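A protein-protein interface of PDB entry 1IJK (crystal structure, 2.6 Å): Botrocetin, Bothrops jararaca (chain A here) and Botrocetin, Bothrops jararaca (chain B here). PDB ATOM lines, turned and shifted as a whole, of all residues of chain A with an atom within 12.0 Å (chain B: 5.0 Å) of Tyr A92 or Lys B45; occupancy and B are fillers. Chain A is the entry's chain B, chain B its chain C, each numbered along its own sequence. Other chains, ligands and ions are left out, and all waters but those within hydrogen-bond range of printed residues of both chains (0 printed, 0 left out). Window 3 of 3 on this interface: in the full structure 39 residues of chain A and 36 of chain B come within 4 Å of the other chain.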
ATOM      1  N   GLU A  77       3.317 -26.110  27.524  1.00  0.00           N
ATOM      2  CA  GLU A  77       4.457 -26.249  26.626  1.00  0.00           C
ATOM      3  C   GLU A  77       5.783 -25.772  27.225  1.00  0.00           C
ATOM      4  O   GLU A  77       5.797 -25.037  28.209  1.00  0.00           O
ATOM      5  CB  GLU A  77       4.175 -25.491  25.336  1.00  0.00           C
ATOM      6  CG  GLU A  77       2.907 -25.929  24.649  1.00  0.00           C
ATOM      7  CD  GLU A  77       1.661 -25.430  25.350  1.00  0.00           C
ATOM      8  OE1 GLU A  77       1.433 -24.196  25.348  1.00  0.00           O
ATOM      9  OE2 GLU A  77       0.911 -26.269  25.902  1.00  0.00           O
ATOM     10  N   LYS A  78       6.891 -26.188  26.615  1.00  0.00           N
ATOM     11  CA  LYS A  78       8.219 -25.804  27.087  1.00  0.00           C
ATOM     12  C   LYS A  78       8.595 -24.384  26.632  1.00  0.00           C
ATOM     13  O   LYS A  78       9.558 -23.797  27.126  1.00  0.00           O
ATOM     14  CB  LYS A  78       9.263 -26.812  26.595  1.00  0.00           C
ATOM     15  CG  LYS A  78       8.818 -28.253  26.758  1.00  0.00           C
ATOM     16  CD  LYS A  78       9.909 -29.254  26.411  1.00  0.00           C
ATOM     17  CE  LYS A  78       9.325 -30.661  26.195  1.00  0.00           C
ATOM     18  NZ  LYS A  78       8.588 -31.222  27.379  1.00  0.00           N
ATOM     19  N   GLN A  79       7.835 -23.850  25.681  1.00  0.00           N
ATOM     20  CA  GLN A  79       8.037 -22.501  25.164  1.00  0.00           C
ATOM     21  C   GLN A  79       6.690 -22.093  24.577  1.00  0.00           C
ATOM     22  O   GLN A  79       6.020 -22.896  23.941  1.00  0.00           O
ATOM     23  CB  GLN A  79       9.176 -22.460  24.119  1.00  0.00           C
ATOM     24  CG  GLN A  79       9.051 -23.364  22.891  1.00  0.00           C
ATOM     25  CD  GLN A  79       8.100 -22.819  21.837  1.00  0.00           C
ATOM     26  OE1 GLN A  79       8.136 -21.632  21.501  1.00  0.00           O
ATOM     27  NE2 GLN A  79       7.251 -23.690  21.300  1.00  0.00           N
ATOM     28  N   CYS A  80       6.292 -20.848  24.788  1.00  0.00           N
ATOM     29  CA  CYS A  80       4.983 -20.408  24.344  1.00  0.00           C
ATOM     30  C   CYS A  80       4.835 -19.812  22.968  1.00  0.00           C
ATOM     31  O   CYS A  80       3.900 -19.046  22.731  1.00  0.00           O
ATOM     32  CB  CYS A  80       4.403 -19.435  25.365  1.00  0.00           C
ATOM     33  SG  CYS A  80       4.791 -19.883  27.082  1.00  0.00           S
ATOM     34  N   SER A  81       5.730 -20.142  22.047  1.00  0.00           N
ATOM     35  CA  SER A  81       5.571 -19.601  20.704  1.00  0.00           C
ATOM     36  C   SER A  81       4.642 -20.558  19.971  1.00  0.00           C
ATOM     37  O   SER A  81       4.933 -21.741  19.840  1.00  0.00           O
ATOM     38  CB  SER A  81       6.914 -19.497  19.980  1.00  0.00           C
ATOM     39  OG  SER A  81       6.842 -18.527  18.951  1.00  0.00           O
ATOM     40  N   SER A  82       3.506 -20.033  19.528  1.00  0.00           N
ATOM     41  CA  SER A  82       2.503 -20.817  18.817  1.00  0.00           C
ATOM     42  C   SER A  82       2.947 -21.166  17.402  1.00  0.00           C
ATOM     43  O   SER A  82       2.833 -22.320  16.980  1.00  0.00           O
ATOM     44  CB  SER A  82       1.187 -20.038  18.765  1.00  0.00           C
ATOM     45  OG  SER A  82       0.436 -20.359  17.606  1.00  0.00           O
ATOM     46  N   GLU A  83       3.452 -20.165  16.676  1.00  0.00           N
ATOM     47  CA  GLU A  83       3.904 -20.364  15.298  1.00  0.00           C
ATOM     48  C   GLU A  83       5.350 -19.901  15.083  1.00  0.00           C
ATOM     49  O   GLU A  83       5.912 -19.148  15.896  1.00  0.00           O
ATOM     50  CB  GLU A  83       3.018 -19.580  14.319  1.00  0.00           C
ATOM     51  CG  GLU A  83       1.623 -19.238  14.810  1.00  0.00           C
ATOM     52  CD  GLU A  83       1.211 -17.822  14.412  1.00  0.00           C
ATOM     53  OE1 GLU A  83       1.821 -16.860  14.929  1.00  0.00           O
ATOM     54  OE2 GLU A  83       0.287 -17.663  13.582  1.00  0.00           O
ATOM     55  N   TRP A  84       5.933 -20.347  13.967  1.00  0.00           N
ATOM     56  CA  TRP A  84       7.292 -19.967  13.593  1.00  0.00           C
ATOM     57  C   TRP A  84       7.212 -18.594  12.934  1.00  0.00           C
ATOM     58  O   TRP A  84       6.113 -18.071  12.731  1.00  0.00           O
ATOM     59  CB  TRP A  84       7.888 -20.975  12.614  1.00  0.00           C
ATOM     60  CG  TRP A  84       8.069 -22.342  13.182  1.00  0.00           C
ATOM     61  CD1 TRP A  84       7.118 -23.303  13.315  1.00  0.00           C
ATOM     62  CD2 TRP A  84       9.295 -22.920  13.647  1.00  0.00           C
ATOM     63  NE1 TRP A  84       7.674 -24.453  13.828  1.00  0.00           N
ATOM     64  CE2 TRP A  84       9.009 -24.243  14.043  1.00  0.00           C
ATOM     65  CE3 TRP A  84      10.607 -22.445  13.767  1.00  0.00           C
ATOM     66  CZ2 TRP A  84       9.981 -25.098  14.549  1.00  0.00           C
ATOM     67  CZ3 TRP A  84      11.574 -23.291  14.268  1.00  0.00           C
ATOM     68  CH2 TRP A  84      11.257 -24.608  14.656  1.00  0.00           C
ATOM     69  N   SER A  85       8.353 -18.004  12.591  1.00  0.00           N
ATOM     70  CA  SER A  85       8.310 -16.682  11.985  1.00  0.00           C
ATOM     71  C   SER A  85       7.642 -16.693  10.620  1.00  0.00           C
ATOM     72  O   SER A  85       7.260 -15.643  10.110  1.00  0.00           O
ATOM     73  CB  SER A  85       9.710 -16.066  11.891  1.00  0.00           C
ATOM     74  OG  SER A  85      10.609 -16.891  11.181  1.00  0.00           O
ATOM     75  N   ASP A  86       7.503 -17.866  10.014  1.00  0.00           N
ATOM     76  CA  ASP A  86       6.825 -17.929   8.719  1.00  0.00           C
ATOM     77  C   ASP A  86       5.322 -17.789   8.985  1.00  0.00           C
ATOM     78  O   ASP A  86       4.715 -16.762   8.677  1.00  0.00           O
ATOM     79  CB  ASP A  86       7.130 -19.247   7.979  1.00  0.00           C
ATOM     80  CG  ASP A  86       7.106 -20.472   8.894  1.00  0.00           C
ATOM     81  OD1 ASP A  86       6.157 -20.612   9.701  1.00  0.00           O
ATOM     82  OD2 ASP A  86       8.038 -21.313   8.787  1.00  0.00           O
ATOM     83  N   GLY A  87       4.741 -18.816   9.593  1.00  0.00           N
ATOM     84  CA  GLY A  87       3.329 -18.803   9.915  1.00  0.00           C
ATOM     85  C   GLY A  87       2.927 -20.189  10.379  1.00  0.00           C
ATOM     86  O   GLY A  87       1.932 -20.370  11.087  1.00  0.00           O
ATOM     87  N   SER A  88       3.711 -21.177   9.976  1.00  0.00           N
ATOM     88  CA  SER A  88       3.425 -22.542  10.353  1.00  0.00           C
ATOM     89  C   SER A  88       3.248 -22.668  11.858  1.00  0.00           C
ATOM     90  O   SER A  88       4.040 -22.135  12.641  1.00  0.00           O
ATOM     91  CB  SER A  88       4.553 -23.464   9.889  1.00  0.00           C
ATOM     92  OG  SER A  88       5.805 -23.030  10.381  1.00  0.00           O
ATOM     93  N   SER A  89       2.191 -23.361  12.264  1.00  0.00           N
ATOM     94  CA  SER A  89       1.947 -23.582  13.682  1.00  0.00           C
ATOM     95  C   SER A  89       3.109 -24.426  14.201  1.00  0.00           C
ATOM     96  O   SER A  89       3.853 -25.019  13.418  1.00  0.00           O
ATOM     97  CB  SER A  89       0.630 -24.331  13.875  1.00  0.00           C
ATOM     98  OG  SER A  89       0.605 -25.502  13.078  1.00  0.00           O
ATOM     99  N   VAL A  90       3.282 -24.473  15.514  1.00  0.00           N
ATOM    100  CA  VAL A  90       4.363 -25.268  16.076  1.00  0.00           C
ATOM    101  C   VAL A  90       3.744 -26.538  16.632  1.00  0.00           C
ATOM    102  O   VAL A  90       2.656 -26.507  17.200  1.00  0.00           O
ATOM    103  CB  VAL A  90       5.107 -24.513  17.212  1.00  0.00           C
ATOM    104  CG1 VAL A  90       6.321 -25.318  17.675  1.00  0.00           C
ATOM    105  CG2 VAL A  90       5.547 -23.145  16.723  1.00  0.00           C
ATOM    106  N   SER A  91       4.425 -27.660  16.447  1.00  0.00           N
ATOM    107  CA  SER A  91       3.932 -28.931  16.947  1.00  0.00           C
ATOM    108  C   SER A  91       5.160 -29.791  17.181  1.00  0.00           C
ATOM    109  O   SER A  91       5.320 -30.381  18.252  1.00  0.00           O
ATOM    110  CB  SER A  91       2.988 -29.583  15.931  1.00  0.00           C
ATOM    111  OG  SER A  91       2.071 -30.465  16.570  1.00  0.00           O
ATOM    112  N   TYR A  92       6.036 -29.867  16.185  1.00  0.00           N
ATOM    113  CA  TYR A  92       7.261 -30.628  16.368  1.00  0.00           C
ATOM    114  C   TYR A  92       8.189 -29.734  17.189  1.00  0.00           C
ATOM    115  O   TYR A  92       8.547 -28.642  16.758  1.00  0.00           O
ATOM    116  CB  TYR A  92       7.921 -30.962  15.030  1.00  0.00           C
ATOM    117  CG  TYR A  92       9.308 -31.559  15.183  1.00  0.00           C
ATOM    118  CD1 TYR A  92       9.519 -32.701  15.956  1.00  0.00           C
ATOM    119  CD2 TYR A  92      10.405 -30.982  14.552  1.00  0.00           C
ATOM    120  CE1 TYR A  92      10.790 -33.255  16.093  1.00  0.00           C
ATOM    121  CE2 TYR A  92      11.679 -31.523  14.680  1.00  0.00           C
ATOM    122  CZ  TYR A  92      11.867 -32.662  15.448  1.00  0.00           C
ATOM    123  OH  TYR A  92      13.131 -33.212  15.549  1.00  0.00           O
ATOM    124  N   GLU A  93       8.561 -30.197  18.376  1.00  0.00           N
ATOM    125  CA  GLU A  93       9.430 -29.431  19.257  1.00  0.00           C
ATOM    126  C   GLU A  93      10.629 -30.296  19.646  1.00  0.00           C
ATOM    127  O   GLU A  93      10.582 -31.519  19.537  1.00  0.00           O
ATOM    128  CB  GLU A  93       8.642 -29.001  20.507  1.00  0.00           C
ATOM    129  CG  GLU A  93       9.341 -27.994  21.411  1.00  0.00           C
ATOM    130  CD  GLU A  93       8.401 -27.379  22.456  1.00  0.00           C
ATOM    131  OE1 GLU A  93       7.921 -28.120  23.344  1.00  0.00           O
ATOM    132  OE2 GLU A  93       8.139 -26.154  22.391  1.00  0.00           O
ATOM    133  N   ASN A  94      11.706 -29.657  20.081  1.00  0.00           N
ATOM    134  CA  ASN A  94      12.896 -30.382  20.494  1.00  0.00           C
ATOM    135  C   ASN A  94      13.714 -29.474  21.414  1.00  0.00           C
ATOM    136  O   ASN A  94      14.934 -29.376  21.290  1.00  0.00           O
ATOM    137  CB  ASN A  94      13.708 -30.787  19.265  1.00  0.00           C
ATOM    138  CG  ASN A  94      14.669 -31.932  19.545  1.00  0.00           C
ATOM    139  OD1 ASN A  94      15.417 -32.351  18.662  1.00  0.00           O
ATOM    140  ND2 ASN A  94      14.650 -32.447  20.771  1.00  0.00           N
ATOM    141  N   VAL A  95      13.014 -28.829  22.346  1.00  0.00           N
ATOM    142  CA  VAL A  95      13.603 -27.898  23.310  1.00  0.00           C
ATOM    143  C   VAL A  95      14.280 -28.551  24.524  1.00  0.00           C
ATOM    144  O   VAL A  95      13.726 -29.454  25.159  1.00  0.00           O
ATOM    145  CB  VAL A  95      12.526 -26.904  23.835  1.00  0.00           C
ATOM    146  CG1 VAL A  95      13.131 -25.969  24.860  1.00  0.00           C
ATOM    147  CG2 VAL A  95      11.943 -26.113  22.679  1.00  0.00           C
ATOM    148  N   VAL A  96      15.477 -28.065  24.838  1.00  0.00           N
ATOM    149  CA  VAL A  96      16.264 -28.541  25.970  1.00  0.00           C
ATOM    150  C   VAL A  96      15.640 -28.028  27.280  1.00  0.00           C
ATOM    151  O   VAL A  96      15.598 -26.822  27.528  1.00  0.00           O
ATOM    152  CB  VAL A  96      17.712 -28.024  25.857  1.00  0.00           C
ATOM    153  CG1 VAL A  96      18.536 -28.484  27.037  1.00  0.00           C
ATOM    154  CG2 VAL A  96      18.324 -28.500  24.557  1.00  0.00           C
ATOM    155  N   PHE B  42      11.194 -25.969  11.466  1.00  0.00           N
ATOM    156  CA  PHE B  42      11.071 -27.424  11.363  1.00  0.00           C
ATOM    157  C   PHE B  42       9.657 -27.903  11.667  1.00  0.00           C
ATOM    158  O   PHE B  42       9.156 -27.709  12.775  1.00  0.00           O
ATOM    159  CB  PHE B  42      12.046 -28.120  12.326  1.00  0.00           C
ATOM    160  CG  PHE B  42      13.483 -27.704  12.161  1.00  0.00           C
ATOM    161  CD1 PHE B  42      14.451 -28.161  13.053  1.00  0.00           C
ATOM    162  CD2 PHE B  42      13.876 -26.858  11.127  1.00  0.00           C
ATOM    163  CE1 PHE B  42      15.792 -27.782  12.924  1.00  0.00           C
ATOM    164  CE2 PHE B  42      15.210 -26.474  10.988  1.00  0.00           C
ATOM    165  CZ  PHE B  42      16.170 -26.936  11.889  1.00  0.00           C
ATOM    166  N   GLN B  43       9.021 -28.535  10.686  1.00  0.00           N
ATOM    167  CA  GLN B  43       7.669 -29.047  10.866  1.00  0.00           C
ATOM    168  C   GLN B  43       7.714 -30.570  11.068  1.00  0.00           C
ATOM    169  O   GLN B  43       6.680 -31.236  11.128  1.00  0.00           O
ATOM    170  CB  GLN B  43       6.810 -28.708   9.648  1.00  0.00           C
ATOM    171  CG  GLN B  43       6.968 -27.281   9.116  1.00  0.00           C
ATOM    172  CD  GLN B  43       6.520 -26.207  10.096  1.00  0.00           C
ATOM    173  OE1 GLN B  43       5.512 -26.358  10.792  1.00  0.00           O
ATOM    174  NE2 GLN B  43       7.258 -25.103  10.136  1.00  0.00           N
ATOM    175  N   SER B  44       8.925 -31.108  11.183  1.00  0.00           N
ATOM    176  CA  SER B  44       9.141 -32.543  11.380  1.00  0.00           C
ATOM    177  C   SER B  44      10.642 -32.798  11.541  1.00  0.00           C
ATOM    178  O   SER B  44      11.455 -31.958  11.158  1.00  0.00           O
ATOM    179  CB  SER B  44       8.604 -33.329  10.175  1.00  0.00           C
ATOM    180  OG  SER B  44       9.155 -32.857   8.951  1.00  0.00           O
ATOM    181  N   LYS B  45      11.025 -33.942  12.101  1.00  0.00           N
ATOM    182  CA  LYS B  45      12.450 -34.204  12.256  1.00  0.00           C
ATOM    183  C   LYS B  45      13.160 -34.165  10.910  1.00  0.00           C
ATOM    184  O   LYS B  45      14.165 -33.476  10.753  1.00  0.00           O
ATOM    185  CB  LYS B  45      12.717 -35.560  12.909  1.00  0.00           C
ATOM    186  CG  LYS B  45      14.213 -35.869  12.992  1.00  0.00           C
ATOM    187  CD  LYS B  45      14.499 -37.162  13.728  1.00  0.00           C
ATOM    188  CE  LYS B  45      15.998 -37.434  13.801  1.00  0.00           C
ATOM    189  NZ  LYS B  45      16.734 -36.329  14.470  1.00  0.00           N
ATOM    190  N   GLU B  46      12.634 -34.909   9.943  1.00  0.00           N
ATOM    191  CA  GLU B  46      13.225 -34.963   8.611  1.00  0.00           C
ATOM    192  C   GLU B  46      13.733 -33.602   8.140  1.00  0.00           C
ATOM    193  O   GLU B  46      14.881 -33.487   7.706  1.00  0.00           O
ATOM    194  CB  GLU B  46      12.210 -35.517   7.602  1.00  0.00           C
ATOM    195  CG  GLU B  46      12.002 -37.033   7.653  1.00  0.00           C
ATOM    196  CD  GLU B  46      11.698 -37.558   9.049  1.00  0.00           C
ATOM    197  OE1 GLU B  46      12.648 -37.737   9.843  1.00  0.00           O
ATOM    198  OE2 GLU B  46      10.506 -37.788   9.355  1.00  0.00           O
ATOM    199  N   GLU B  47      12.885 -32.578   8.232  1.00  0.00           N
ATOM    200  CA  GLU B  47      13.265 -31.229   7.802  1.00  0.00           C
ATOM    201  C   GLU B  47      14.528 -30.763   8.525  1.00  0.00           C
ATOM    202  O   GLU B  47      15.369 -30.081   7.945  1.00  0.00           O
ATOM    203  CB  GLU B  47      12.122 -30.233   8.057  1.00  0.00           C
ATOM    204  CG  GLU B  47      12.340 -28.867   7.411  1.00  0.00           C
ATOM    205  CD  GLU B  47      11.156 -27.923   7.583  1.00  0.00           C
ATOM    206  OE1 GLU B  47      11.215 -26.772   7.091  1.00  0.00           O
ATOM    207  OE2 GLU B  47      10.161 -28.330   8.213  1.00  0.00           O
ATOM    208  N   ALA B  48      14.659 -31.143   9.790  1.00  0.00           N
ATOM    209  CA  ALA B  48      15.819 -30.764  10.588  1.00  0.00           C
ATOM    210  C   ALA B  48      17.093 -31.353  10.009  1.00  0.00           C
ATOM    211  O   ALA B  48      18.098 -30.657   9.854  1.00  0.00           O
ATOM    212  CB  ALA B  48      15.639 -31.235  12.030  1.00  0.00           C
ATOM    213  N   ASP B  49      17.037 -32.646   9.693  1.00  0.00           N
ATOM    214  CA  ASP B  49      18.170 -33.384   9.141  1.00  0.00           C
ATOM    215  C   ASP B  49      18.760 -32.690   7.913  1.00  0.00           C
ATOM    216  O   ASP B  49      19.979 -32.539   7.795  1.00  0.00           O
ATOM    217  CB  ASP B  49      17.725 -34.800   8.778  1.00  0.00           C
ATOM    218  CG  ASP B  49      17.016 -35.498   9.925  1.00  0.00           C
ATOM    219  OD1 ASP B  49      15.950 -35.009  10.352  1.00  0.00           O
ATOM    220  OD2 ASP B  49      17.521 -36.536  10.404  1.00  0.00           O
ATOM    221  N   ASN B 106      20.863 -31.956  17.498  1.00  0.00           N
ATOM    222  CA  ASN B 106      19.577 -31.470  17.025  1.00  0.00           C
ATOM    223  C   ASN B 106      18.652 -31.063  18.168  1.00  0.00           C
ATOM    224  O   ASN B 106      17.430 -31.177  18.055  1.00  0.00           O
ATOM    225  CB  ASN B 106      18.892 -32.527  16.160  1.00  0.00           C
ATOM    226  CG  ASN B 106      17.549 -32.067  15.645  1.00  0.00           C
ATOM    227  OD1 ASN B 106      17.444 -31.017  15.009  1.00  0.00           O
ATOM    228  ND2 ASN B 106      16.505 -32.843  15.926  1.00  0.00           N
ATOM    229  N   TRP B 108      17.161 -28.093  20.629  1.00  0.00           N
ATOM    230  CA  TRP B 108      16.942 -26.652  20.593  1.00  0.00           C
ATOM    231  C   TRP B 108      17.231 -25.985  21.928  1.00  0.00           C
ATOM    232  O   TRP B 108      16.886 -26.510  22.986  1.00  0.00           O
ATOM    233  CB  TRP B 108      15.500 -26.339  20.188  1.00  0.00           C
ATOM    234  CG  TRP B 108      15.048 -27.029  18.939  1.00  0.00           C
ATOM    235  CD1 TRP B 108      15.772 -27.894  18.169  1.00  0.00           C
ATOM    236  CD2 TRP B 108      13.755 -26.930  18.323  1.00  0.00           C
ATOM    237  NE1 TRP B 108      15.013 -28.339  17.117  1.00  0.00           N
ATOM    238  CE2 TRP B 108      13.772 -27.763  17.184  1.00  0.00           C
ATOM    239  CE3 TRP B 108      12.586 -26.216  18.622  1.00  0.00           C
ATOM    240  CZ2 TRP B 108      12.663 -27.905  16.340  1.00  0.00           C
ATOM    241  CZ3 TRP B 108      11.482 -26.355  17.781  1.00  0.00           C
ATOM    242  CH2 TRP B 108      11.531 -27.195  16.653  1.00  0.00           C
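OD1 of Asn A94 sits close to O of Asn B106, at 2.4 Å. The side-chain amide oxygen (OE1) of Gln B43 sits close to the backbone carbonyl oxygen (O) of Ser A89 (3.4 Å). The side-chain hydroxyl (OH) of Tyr A92 lies within hydrogen-bond range of the side-chain amide nitrogen (ND2) of Asn B106 (3.4 Å). N of Trp B108 is in hydrogen-bond range of O of Asn A94 (2.7 Å). The side-chain hydroxyl of Ser A88 is in hydrogen-bond range of the side-chain amide nitrogen of Gln B43 (2.5 Å). O of Trp B108 sits at hydrogen-bond distance from N of Val A96 (2.8 Å).
OE2 of Glu A93 is in hydrogen-bond range of NE2 of Gln A79. N of Gln B43 is in hydrogen-bond range of OE2 of Glu B47, 2.7 Å away. The side-chain carboxylate (OD1) of Asp A86 is in hydrogen-bond range of the backbone NH (N) of Ser A88.
CZ2 of Trp A84 touches O of Phe B42, 3.3 Å away. Gln B43 touches Trp A84. Trp A84 touches Trp B108 (CH2 to CH2, 3.3 Å). O of Phe B42 touches CD2 of Tyr A92, 3.9 Å away. Gln B43 touches Tyr A92 (C to CB, 3.99 Å). Tyr A92 touches Ser B44. Tyr A92 touches Lys B45 (OH to CA, 3.5 Å). Trp B108 touches Tyr A92. Trp B108 touches Glu A93. Trp B108 touches Val A95.
Of the printed residues of chain B, Tyr A92 touches Phe B42, Gln B43, Ser B44, Lys B45, Asn B106 and Trp B108. Lys B45 touches just one residue of chain A: Tyr A92. Phe B42 touches just these residues of chain A: Trp A84 and Tyr A92. No residue of chain A comes within 4 Å of Ala B48. No residue of chain A comes within 4 Å of Asp B49. Asn B106 touches just these residues of chain A: Tyr A92 and Asn A94. Printed residues of chain B within 4 Å of Asn A94: Asn B106 (2.4 Å) and Trp B108 (2.7 Å). Of the printed residues of chain B, Ser A88 touches Gln B43 (2.5 Å). Of the printed residues of chain B, Val A95 touches Trp B108 (3.6 Å). Val A90 touches none of the printed residues of chain B. Gln A79 touches none of the printed residues of chain B. The nearest residue of chain A that does not touch Lys B45 is Asn A94 (5.9 Å). The nearest printed residue of chain B that does not touch Val A95 is Asn B106 (6.6 Å).
Printed residues of chain B that touch a printed residue of chain A: Phe B42, Gln B43, Ser B44, Lys B45, Asn B106 and Trp B108. Hydrophobic or aromatic side chains of chain B within 4 Å of the printed part of chain A: Phe B42 and Trp B108. Among the printed residues, 16 pairs touch across the chains. Among the printed residues, no Asp or Glu carboxylate lies within 4 Å of a Lys or Arg side-chain nitrogen of the other chain.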
